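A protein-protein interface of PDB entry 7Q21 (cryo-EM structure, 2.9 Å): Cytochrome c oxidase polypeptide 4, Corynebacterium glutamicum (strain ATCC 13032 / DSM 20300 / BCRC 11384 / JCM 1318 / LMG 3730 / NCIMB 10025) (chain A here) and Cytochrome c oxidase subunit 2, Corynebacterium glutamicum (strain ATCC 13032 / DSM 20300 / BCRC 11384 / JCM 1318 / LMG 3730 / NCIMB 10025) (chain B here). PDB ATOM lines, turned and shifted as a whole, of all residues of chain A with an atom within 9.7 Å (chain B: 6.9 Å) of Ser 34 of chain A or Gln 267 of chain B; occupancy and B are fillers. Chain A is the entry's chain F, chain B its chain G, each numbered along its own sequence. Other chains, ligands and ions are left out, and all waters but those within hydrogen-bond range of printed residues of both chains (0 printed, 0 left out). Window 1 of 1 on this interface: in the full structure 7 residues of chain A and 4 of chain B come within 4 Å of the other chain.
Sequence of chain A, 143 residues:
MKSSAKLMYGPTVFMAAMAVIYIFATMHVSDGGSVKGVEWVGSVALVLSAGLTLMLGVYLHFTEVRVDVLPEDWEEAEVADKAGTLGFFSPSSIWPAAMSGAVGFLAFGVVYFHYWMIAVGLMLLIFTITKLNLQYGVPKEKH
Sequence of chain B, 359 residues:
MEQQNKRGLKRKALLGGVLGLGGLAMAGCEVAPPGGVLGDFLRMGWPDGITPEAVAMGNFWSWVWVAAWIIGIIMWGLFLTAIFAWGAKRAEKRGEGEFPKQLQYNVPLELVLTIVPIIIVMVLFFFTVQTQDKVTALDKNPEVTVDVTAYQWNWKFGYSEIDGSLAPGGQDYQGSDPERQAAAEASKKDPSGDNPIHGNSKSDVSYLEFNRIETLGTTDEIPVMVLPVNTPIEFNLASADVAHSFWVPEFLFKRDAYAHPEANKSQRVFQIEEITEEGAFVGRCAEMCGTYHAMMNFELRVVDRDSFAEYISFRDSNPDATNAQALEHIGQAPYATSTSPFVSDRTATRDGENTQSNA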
ATOM      1  N   TYR A  22      11.136  22.709 -11.418  1.00  0.00           N
ATOM      2  CA  TYR A  22      10.845  21.293 -11.263  1.00  0.00           C
ATOM      3  C   TYR A  22      11.561  20.700 -10.051  1.00  0.00           C
ATOM      4  O   TYR A  22      10.938  20.029  -9.232  1.00  0.00           O
ATOM      5  CB  TYR A  22      11.154  20.520 -12.543  1.00  0.00           C
ATOM      6  CG  TYR A  22      10.588  19.127 -12.556  1.00  0.00           C
ATOM      7  CD1 TYR A  22      11.418  18.026 -12.667  1.00  0.00           C
ATOM      8  CD2 TYR A  22       9.221  18.909 -12.457  1.00  0.00           C
ATOM      9  CE1 TYR A  22      10.905  16.738 -12.702  1.00  0.00           C
ATOM     10  CE2 TYR A  22       8.691  17.628 -12.476  1.00  0.00           C
ATOM     11  CZ  TYR A  22       9.538  16.538 -12.596  1.00  0.00           C
ATOM     12  OH  TYR A  22       9.014  15.280 -12.615  1.00  0.00           O
ATOM     13  N   ALA A  25      10.250  22.211  -6.751  1.00  0.00           N
ATOM     14  CA  ALA A  25       8.853  21.907  -6.477  1.00  0.00           C
ATOM     15  C   ALA A  25       8.652  20.416  -6.208  1.00  0.00           C
ATOM     16  O   ALA A  25       7.639  20.035  -5.627  1.00  0.00           O
ATOM     17  CB  ALA A  25       7.967  22.397  -7.602  1.00  0.00           C
ATOM     18  N   THR A  26       9.600  19.571  -6.630  1.00  0.00           N
ATOM     19  CA  THR A  26       9.486  18.135  -6.404  1.00  0.00           C
ATOM     20  C   THR A  26      10.041  17.750  -5.033  1.00  0.00           C
ATOM     21  O   THR A  26       9.637  16.732  -4.477  1.00  0.00           O
ATOM     22  CB  THR A  26      10.142  17.309  -7.516  1.00  0.00           C
ATOM     23  OG1 THR A  26      11.442  17.840  -7.770  1.00  0.00           O
ATOM     24  CG2 THR A  26       9.330  17.293  -8.790  1.00  0.00           C
ATOM     25  N   MET A  27      10.959  18.561  -4.497  1.00  0.00           N
ATOM     26  CA  MET A  27      11.656  18.203  -3.274  1.00  0.00           C
ATOM     27  C   MET A  27      11.086  18.940  -2.059  1.00  0.00           C
ATOM     28  O   MET A  27      11.532  18.684  -0.939  1.00  0.00           O
ATOM     29  CB  MET A  27      13.161  18.460  -3.398  1.00  0.00           C
ATOM     30  CG  MET A  27      13.559  19.922  -3.280  1.00  0.00           C
ATOM     31  SD  MET A  27      15.276  20.156  -2.763  1.00  0.00           S
ATOM     32  CE  MET A  27      16.126  19.788  -4.296  1.00  0.00           C
ATOM     33  N   HIS A  28      10.092  19.818  -2.272  1.00  0.00           N
ATOM     34  CA  HIS A  28       9.596  20.659  -1.191  1.00  0.00           C
ATOM     35  C   HIS A  28       8.071  20.805  -1.241  1.00  0.00           C
ATOM     36  O   HIS A  28       7.483  21.661  -0.579  1.00  0.00           O
ATOM     37  CB  HIS A  28      10.375  21.989  -1.166  1.00  0.00           C
ATOM     38  CG  HIS A  28      10.170  22.796   0.071  1.00  0.00           C
ATOM     39  ND1 HIS A  28       9.098  23.651   0.210  1.00  0.00           N
ATOM     40  CD2 HIS A  28      10.881  22.889   1.217  1.00  0.00           C
ATOM     41  CE1 HIS A  28       9.148  24.234   1.390  1.00  0.00           C
ATOM     42  NE2 HIS A  28      10.236  23.785   2.027  1.00  0.00           N
ATOM     43  N   VAL A  29       7.403  19.971  -2.049  1.00  0.00           N
ATOM     44  CA  VAL A  29       5.948  20.015  -2.117  1.00  0.00           C
ATOM     45  C   VAL A  29       5.389  18.638  -1.783  1.00  0.00           C
ATOM     46  O   VAL A  29       5.772  17.649  -2.403  1.00  0.00           O
ATOM     47  CB  VAL A  29       5.428  20.554  -3.468  1.00  0.00           C
ATOM     48  CG1 VAL A  29       3.929  20.360  -3.626  1.00  0.00           C
ATOM     49  CG2 VAL A  29       5.807  22.014  -3.682  1.00  0.00           C
ATOM     50  N   SER A  30       4.479  18.604  -0.803  1.00  0.00           N
ATOM     51  CA  SER A  30       3.702  17.417  -0.488  1.00  0.00           C
ATOM     52  C   SER A  30       2.267  17.616  -0.968  1.00  0.00           C
ATOM     53  O   SER A  30       1.559  18.490  -0.466  1.00  0.00           O
ATOM     54  CB  SER A  30       3.760  17.109   0.987  1.00  0.00           C
ATOM     55  OG  SER A  30       5.084  16.802   1.388  1.00  0.00           O
ATOM     56  N   ASP A  31       1.853  16.796  -1.943  1.00  0.00           N
ATOM     57  CA  ASP A  31       0.542  16.936  -2.557  1.00  0.00           C
ATOM     58  C   ASP A  31      -0.449  15.940  -1.959  1.00  0.00           C
ATOM     59  O   ASP A  31      -1.645  16.227  -1.896  1.00  0.00           O
ATOM     60  CB  ASP A  31       0.597  16.819  -4.082  1.00  0.00           C
ATOM     61  CG  ASP A  31      -0.742  17.123  -4.735  1.00  0.00           C
ATOM     62  OD1 ASP A  31      -1.075  18.317  -4.867  1.00  0.00           O
ATOM     63  OD2 ASP A  31      -1.458  16.162  -5.068  1.00  0.00           O
ATOM     64  N   GLY A  32       0.059  14.771  -1.548  1.00  0.00           N
ATOM     65  CA  GLY A  32      -0.778  13.679  -1.075  1.00  0.00           C
ATOM     66  C   GLY A  32      -1.082  12.669  -2.181  1.00  0.00           C
ATOM     67  O   GLY A  32      -1.343  11.498  -1.904  1.00  0.00           O
ATOM     68  N   GLY A  33      -1.047  13.140  -3.434  1.00  0.00           N
ATOM     69  CA  GLY A  33      -1.180  12.287  -4.604  1.00  0.00           C
ATOM     70  C   GLY A  33       0.179  11.960  -5.216  1.00  0.00           C
ATOM     71  O   GLY A  33       0.244  11.536  -6.369  1.00  0.00           O
ATOM     72  N   SER A  34       1.245  12.188  -4.438  1.00  0.00           N
ATOM     73  CA  SER A  34       2.617  11.849  -4.777  1.00  0.00           C
ATOM     74  C   SER A  34       3.453  11.799  -3.500  1.00  0.00           C
ATOM     75  O   SER A  34       2.946  12.050  -2.406  1.00  0.00           O
ATOM     76  CB  SER A  34       3.198  12.822  -5.777  1.00  0.00           C
ATOM     77  OG  SER A  34       3.345  14.112  -5.202  1.00  0.00           O
ATOM     78  N   VAL A  35       4.740  11.481  -3.661  1.00  0.00           N
ATOM     79  CA  VAL A  35       5.643  11.359  -2.524  1.00  0.00           C
ATOM     80  C   VAL A  35       6.731  12.415  -2.701  1.00  0.00           C
ATOM     81  O   VAL A  35       7.205  12.620  -3.817  1.00  0.00           O
ATOM     82  CB  VAL A  35       6.228   9.931  -2.386  1.00  0.00           C
ATOM     83  CG1 VAL A  35       7.162   9.801  -1.193  1.00  0.00           C
ATOM     84  CG2 VAL A  35       5.162   8.841  -2.315  1.00  0.00           C
ATOM     85  N   LYS A  36       7.120  13.071  -1.601  1.00  0.00           N
ATOM     86  CA  LYS A  36       8.166  14.080  -1.617  1.00  0.00           C
ATOM     87  C   LYS A  36       9.479  13.449  -2.084  1.00  0.00           C
ATOM     88  O   LYS A  36       9.781  12.311  -1.732  1.00  0.00           O
ATOM     89  CB  LYS A  36       8.297  14.689  -0.222  1.00  0.00           C
ATOM     90  CG  LYS A  36       9.173  15.932  -0.140  1.00  0.00           C
ATOM     91  CD  LYS A  36       9.365  16.485   1.243  1.00  0.00           C
ATOM     92  CE  LYS A  36       8.299  17.492   1.616  1.00  0.00           C
ATOM     93  NZ  LYS A  36       8.351  17.848   3.054  1.00  0.00           N
ATOM     94  N   GLY A  37      10.240  14.203  -2.879  1.00  0.00           N
ATOM     95  CA  GLY A  37      11.559  13.787  -3.330  1.00  0.00           C
ATOM     96  C   GLY A  37      11.836  14.281  -4.746  1.00  0.00           C
ATOM     97  O   GLY A  37      10.920  14.381  -5.565  1.00  0.00           O
ATOM     98  N   GLU A  39      12.777  14.273  -8.510  1.00  0.00           N
ATOM     99  CA  GLU A  39      12.353  13.346  -9.546  1.00  0.00           C
ATOM    100  C   GLU A  39      13.524  12.596 -10.182  1.00  0.00           C
ATOM    101  O   GLU A  39      13.421  11.401 -10.434  1.00  0.00           O
ATOM    102  CB  GLU A  39      11.533  14.094 -10.592  1.00  0.00           C
ATOM    103  CG  GLU A  39      11.126  13.214 -11.763  1.00  0.00           C
ATOM    104  CD  GLU A  39      10.358  11.968 -11.348  1.00  0.00           C
ATOM    105  OE1 GLU A  39       9.395  12.111 -10.571  1.00  0.00           O
ATOM    106  OE2 GLU A  39      10.737  10.854 -11.780  1.00  0.00           O
ATOM    107  N   THR B 136      -7.054  13.696  -3.108  1.00  0.00           N
ATOM    108  CA  THR B 136      -5.659  13.392  -2.824  1.00  0.00           C
ATOM    109  C   THR B 136      -5.325  13.636  -1.353  1.00  0.00           C
ATOM    110  O   THR B 136      -4.197  13.382  -0.935  1.00  0.00           O
ATOM    111  CB  THR B 136      -4.718  14.157  -3.761  1.00  0.00           C
ATOM    112  OG1 THR B 136      -4.980  15.551  -3.594  1.00  0.00           O
ATOM    113  CG2 THR B 136      -4.863  13.752  -5.213  1.00  0.00           C
ATOM    114  N   LEU B 138      -5.134  12.874   2.554  1.00  0.00           N
ATOM    115  CA  LEU B 138      -4.910  11.646   3.303  1.00  0.00           C
ATOM    116  C   LEU B 138      -5.152  11.872   4.795  1.00  0.00           C
ATOM    117  O   LEU B 138      -4.448  11.306   5.632  1.00  0.00           O
ATOM    118  CB  LEU B 138      -3.481  11.146   3.054  1.00  0.00           C
ATOM    119  CG  LEU B 138      -3.170  10.538   1.685  1.00  0.00           C
ATOM    120  CD1 LEU B 138      -1.917   9.682   1.766  1.00  0.00           C
ATOM    121  CD2 LEU B 138      -4.331   9.715   1.145  1.00  0.00           C
ATOM    122  N   LEU B 237      -2.636  -0.287  -1.911  1.00  0.00           N
ATOM    123  CA  LEU B 237      -2.475  -0.947  -3.198  1.00  0.00           C
ATOM    124  C   LEU B 237      -1.027  -1.376  -3.396  1.00  0.00           C
ATOM    125  O   LEU B 237      -0.105  -0.593  -3.179  1.00  0.00           O
ATOM    126  CB  LEU B 237      -2.881   0.021  -4.314  1.00  0.00           C
ATOM    127  CG  LEU B 237      -4.369   0.114  -4.639  1.00  0.00           C
ATOM    128  CD1 LEU B 237      -5.134   0.857  -3.551  1.00  0.00           C
ATOM    129  CD2 LEU B 237      -4.543   0.830  -5.965  1.00  0.00           C
ATOM    130  N   ARG B 255      -6.417   4.089  -9.593  1.00  0.00           N
ATOM    131  CA  ARG B 255      -5.054   4.283  -9.131  1.00  0.00           C
ATOM    132  C   ARG B 255      -4.214   3.071  -9.514  1.00  0.00           C
ATOM    133  O   ARG B 255      -4.639   1.935  -9.326  1.00  0.00           O
ATOM    134  CB  ARG B 255      -5.028   4.516  -7.617  1.00  0.00           C
ATOM    135  CG  ARG B 255      -3.631   4.516  -7.010  1.00  0.00           C
ATOM    136  CD  ARG B 255      -2.863   5.793  -7.295  1.00  0.00           C
ATOM    137  NE  ARG B 255      -3.449   6.928  -6.588  1.00  0.00           N
ATOM    138  CZ  ARG B 255      -3.125   7.311  -5.355  1.00  0.00           C
ATOM    139  NH1 ARG B 255      -2.202   6.654  -4.675  1.00  0.00           N
ATOM    140  NH2 ARG B 255      -3.726   8.350  -4.803  1.00  0.00           N
ATOM    141  N   ASP B 256      -3.009   3.338 -10.021  1.00  0.00           N
ATOM    142  CA  ASP B 256      -2.064   2.295 -10.377  1.00  0.00           C
ATOM    143  C   ASP B 256      -1.452   1.697  -9.114  1.00  0.00           C
ATOM    144  O   ASP B 256      -1.067   2.425  -8.199  1.00  0.00           O
ATOM    145  CB  ASP B 256      -0.994   2.849 -11.315  1.00  0.00           C
ATOM    146  CG  ASP B 256      -1.441   3.070 -12.747  1.00  0.00           C
ATOM    147  OD1 ASP B 256      -2.671   3.124 -12.983  1.00  0.00           O
ATOM    148  OD2 ASP B 256      -0.551   3.187 -13.615  1.00  0.00           O
ATOM    149  N   PRO B 261       5.995  -0.051  -4.390  1.00  0.00           N
ATOM    150  CA  PRO B 261       5.501   1.310  -4.601  1.00  0.00           C
ATOM    151  C   PRO B 261       6.372   2.383  -3.951  1.00  0.00           C
ATOM    152  O   PRO B 261       6.328   3.534  -4.374  1.00  0.00           O
ATOM    153  CB  PRO B 261       4.106   1.320  -3.958  1.00  0.00           C
ATOM    154  CG  PRO B 261       3.755  -0.136  -3.769  1.00  0.00           C
ATOM    155  CD  PRO B 261       5.073  -0.850  -3.567  1.00  0.00           C
ATOM    156  N   ASN B 264       9.389   3.255  -6.356  1.00  0.00           N
ATOM    157  CA  ASN B 264       8.844   4.003  -7.477  1.00  0.00           C
ATOM    158  C   ASN B 264       8.381   5.391  -7.038  1.00  0.00           C
ATOM    159  O   ASN B 264       8.081   6.231  -7.884  1.00  0.00           O
ATOM    160  CB  ASN B 264       7.722   3.225  -8.163  1.00  0.00           C
ATOM    161  CG  ASN B 264       8.185   1.886  -8.695  1.00  0.00           C
ATOM    162  OD1 ASN B 264       9.380   1.635  -8.806  1.00  0.00           O
ATOM    163  ND2 ASN B 264       7.249   1.007  -9.004  1.00  0.00           N
ATOM    164  N   LYS B 265       8.323   5.615  -5.717  1.00  0.00           N
ATOM    165  CA  LYS B 265       7.901   6.874  -5.118  1.00  0.00           C
ATOM    166  C   LYS B 265       6.468   7.198  -5.534  1.00  0.00           C
ATOM    167  O   LYS B 265       6.144   8.350  -5.823  1.00  0.00           O
ATOM    168  CB  LYS B 265       8.866   8.015  -5.464  1.00  0.00           C
ATOM    169  CG  LYS B 265      10.285   7.882  -4.925  1.00  0.00           C
ATOM    170  CD  LYS B 265      11.192   9.011  -5.372  1.00  0.00           C
ATOM    171  CE  LYS B 265      11.577   8.932  -6.836  1.00  0.00           C
ATOM    172  NZ  LYS B 265      12.186  10.194  -7.316  1.00  0.00           N
ATOM    173  N   SER B 266       5.622   6.161  -5.576  1.00  0.00           N
ATOM    174  CA  SER B 266       4.196   6.318  -5.815  1.00  0.00           C
ATOM    175  C   SER B 266       3.433   6.093  -4.515  1.00  0.00           C
ATOM    176  O   SER B 266       3.689   5.127  -3.798  1.00  0.00           O
ATOM    177  CB  SER B 266       3.710   5.395  -6.905  1.00  0.00           C
ATOM    178  OG  SER B 266       3.469   4.090  -6.400  1.00  0.00           O
ATOM    179  N   GLN B 267       2.494   7.005  -4.236  1.00  0.00           N
ATOM    180  CA  GLN B 267       1.604   6.897  -3.093  1.00  0.00           C
ATOM    181  C   GLN B 267       0.672   5.709  -3.312  1.00  0.00           C
ATOM    182  O   GLN B 267      -0.116   5.702  -4.255  1.00  0.00           O
ATOM    183  CB  GLN B 267       0.819   8.197  -2.917  1.00  0.00           C
ATOM    184  CG  GLN B 267      -0.100   8.187  -1.706  1.00  0.00           C
ATOM    185  CD  GLN B 267       0.620   8.557  -0.432  1.00  0.00           C
ATOM    186  OE1 GLN B 267       0.886   7.714   0.419  1.00  0.00           O
ATOM    187  NE2 GLN B 267       0.939   9.834  -0.289  1.00  0.00           N
ATOM    188  N   ARG B 268       0.780   4.713  -2.427  1.00  0.00           N
ATOM    189  CA  ARG B 268       0.053   3.460  -2.572  1.00  0.00           C
ATOM    190  C   ARG B 268      -1.260   3.500  -1.791  1.00  0.00           C
ATOM    191  O   ARG B 268      -1.972   2.500  -1.735  1.00  0.00           O
ATOM    192  CB  ARG B 268       0.933   2.281  -2.140  1.00  0.00           C
ATOM    193  CG  ARG B 268       1.179   2.187  -0.640  1.00  0.00           C
ATOM    194  CD  ARG B 268       2.211   1.124  -0.329  1.00  0.00           C
ATOM    195  NE  ARG B 268       1.608  -0.158   0.004  1.00  0.00           N
ATOM    196  CZ  ARG B 268       2.216  -1.340  -0.054  1.00  0.00           C
ATOM    197  NH1 ARG B 268       3.472  -1.435  -0.456  1.00  0.00           N
ATOM    198  NH2 ARG B 268       1.552  -2.432   0.282  1.00  0.00           N
ATOM    199  N   VAL B 269      -1.573   4.657  -1.199  1.00  0.00           N
ATOM    200  CA  VAL B 269      -2.716   4.786  -0.311  1.00  0.00           C
ATOM    201  C   VAL B 269      -3.647   5.872  -0.841  1.00  0.00           C
ATOM    202  O   VAL B 269      -3.197   6.951  -1.219  1.00  0.00           O
ATOM    203  CB  VAL B 269      -2.260   5.080   1.131  1.00  0.00           C
ATOM    204  CG1 VAL B 269      -3.351   5.729   1.968  1.00  0.00           C
ATOM    205  CG2 VAL B 269      -1.719   3.837   1.817  1.00  0.00           C
ATOM    206  N   PHE B 270      -4.949   5.568  -0.860  1.00  0.00           N
ATOM    207  CA  PHE B 270      -5.960   6.589  -1.069  1.00  0.00           C
ATOM    208  C   PHE B 270      -7.165   6.307  -0.178  1.00  0.00           C
ATOM    209  O   PHE B 270      -7.447   5.156   0.148  1.00  0.00           O
ATOM    210  CB  PHE B 270      -6.325   6.707  -2.551  1.00  0.00           C
ATOM    211  CG  PHE B 270      -7.221   5.615  -3.076  1.00  0.00           C
ATOM    212  CD1 PHE B 270      -6.686   4.426  -3.555  1.00  0.00           C
ATOM    213  CD2 PHE B 270      -8.601   5.779  -3.100  1.00  0.00           C
ATOM    214  CE1 PHE B 270      -7.514   3.426  -4.048  1.00  0.00           C
ATOM    215  CE2 PHE B 270      -9.428   4.775  -3.587  1.00  0.00           C
ATOM    216  CZ  PHE B 270      -8.882   3.599  -4.057  1.00  0.00           C
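O of Gly 32 of chain A is in hydrogen-bond range of NE2 of Gln 267 of chain B.
Printed residues of chain B that touch a printed residue of chain A: Thr 136, Lys 265, Ser 266 and Gln 267.
Of the 15 printed residues of chain A, 6 touch a printed residue of chain B.
Hydrophobic or aromatic side chains of chain A within 4 Å of the printed part of chain B: Val 35.
Among the printed residues, merely in contact across the chains: Asp 31 of chain A with Thr 136 of chain B, Gly 32 of chain A with Thr 136 of chain B, Gly 33 of chain A with Thr 136 of chain B, Ser 34 of chain A with Gln 267 of chain B, Val 35 of chain A with Lys 265 of chain B, Val 35 of chain A with Ser 266 of chain B, Val 35 of chain A with Gln 267 of chain B and Glu 39 of chain A with Lys 265 of chain B.
Printed residues of chain A within 4 Å of Gln 267 of chain B: Gly 32 (3.3 Å), Ser 34 (3.7 Å) and Val 35 (3.8 Å).
Of chain B, only Thr 136 (3.8 Å) comes within 4 Å of Gly 33 of chain A.
Printed residues of chain A within 4 Å of Ser 266 of chain B: Val 35 (3.9 Å).
No residue of chain A comes within 4 Å of Val 269 of chain B.
Printed residues of chain B within 4 Å of Gly 32 of chain A: Thr 136 and Gln 267.
Printed residues of chain B within 4 Å of Asp 31 of chain A: Thr 136.
Printed residues of chain A within 4 Å of Thr 136 of chain B: Asp 31 (3.8 Å), Gly 32 (3.4 Å) and Gly 33 (3.8 Å).
Printed residues of chain A within 4 Å of Lys 265 of chain B: Val 35 (3.7 Å) and Glu 39 (3.6 Å).
Thr 26 of chain A touches none of the printed residues of chain B.
Arg 255 of chain B touches none of the printed residues of chain A.
The nearest residue of chain B that does not touch Ser 34 of chain A is Lys 265 of chain B (5.0 Å).
The nearest printed residue of chain B that does not touch Glu 39 of chain A is Asn 264 of chain B (6.6 Å).
The backbone NH (N) of Gly 33 of chain A sits close to the side-chain carboxylate (OD2) of Asp 31 of chain A (3.5 Å).
The backbone carbonyl oxygen of Pro 261 of chain B lies within hydrogen-bond range of the backbone NH of Ser 266 of chain B.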
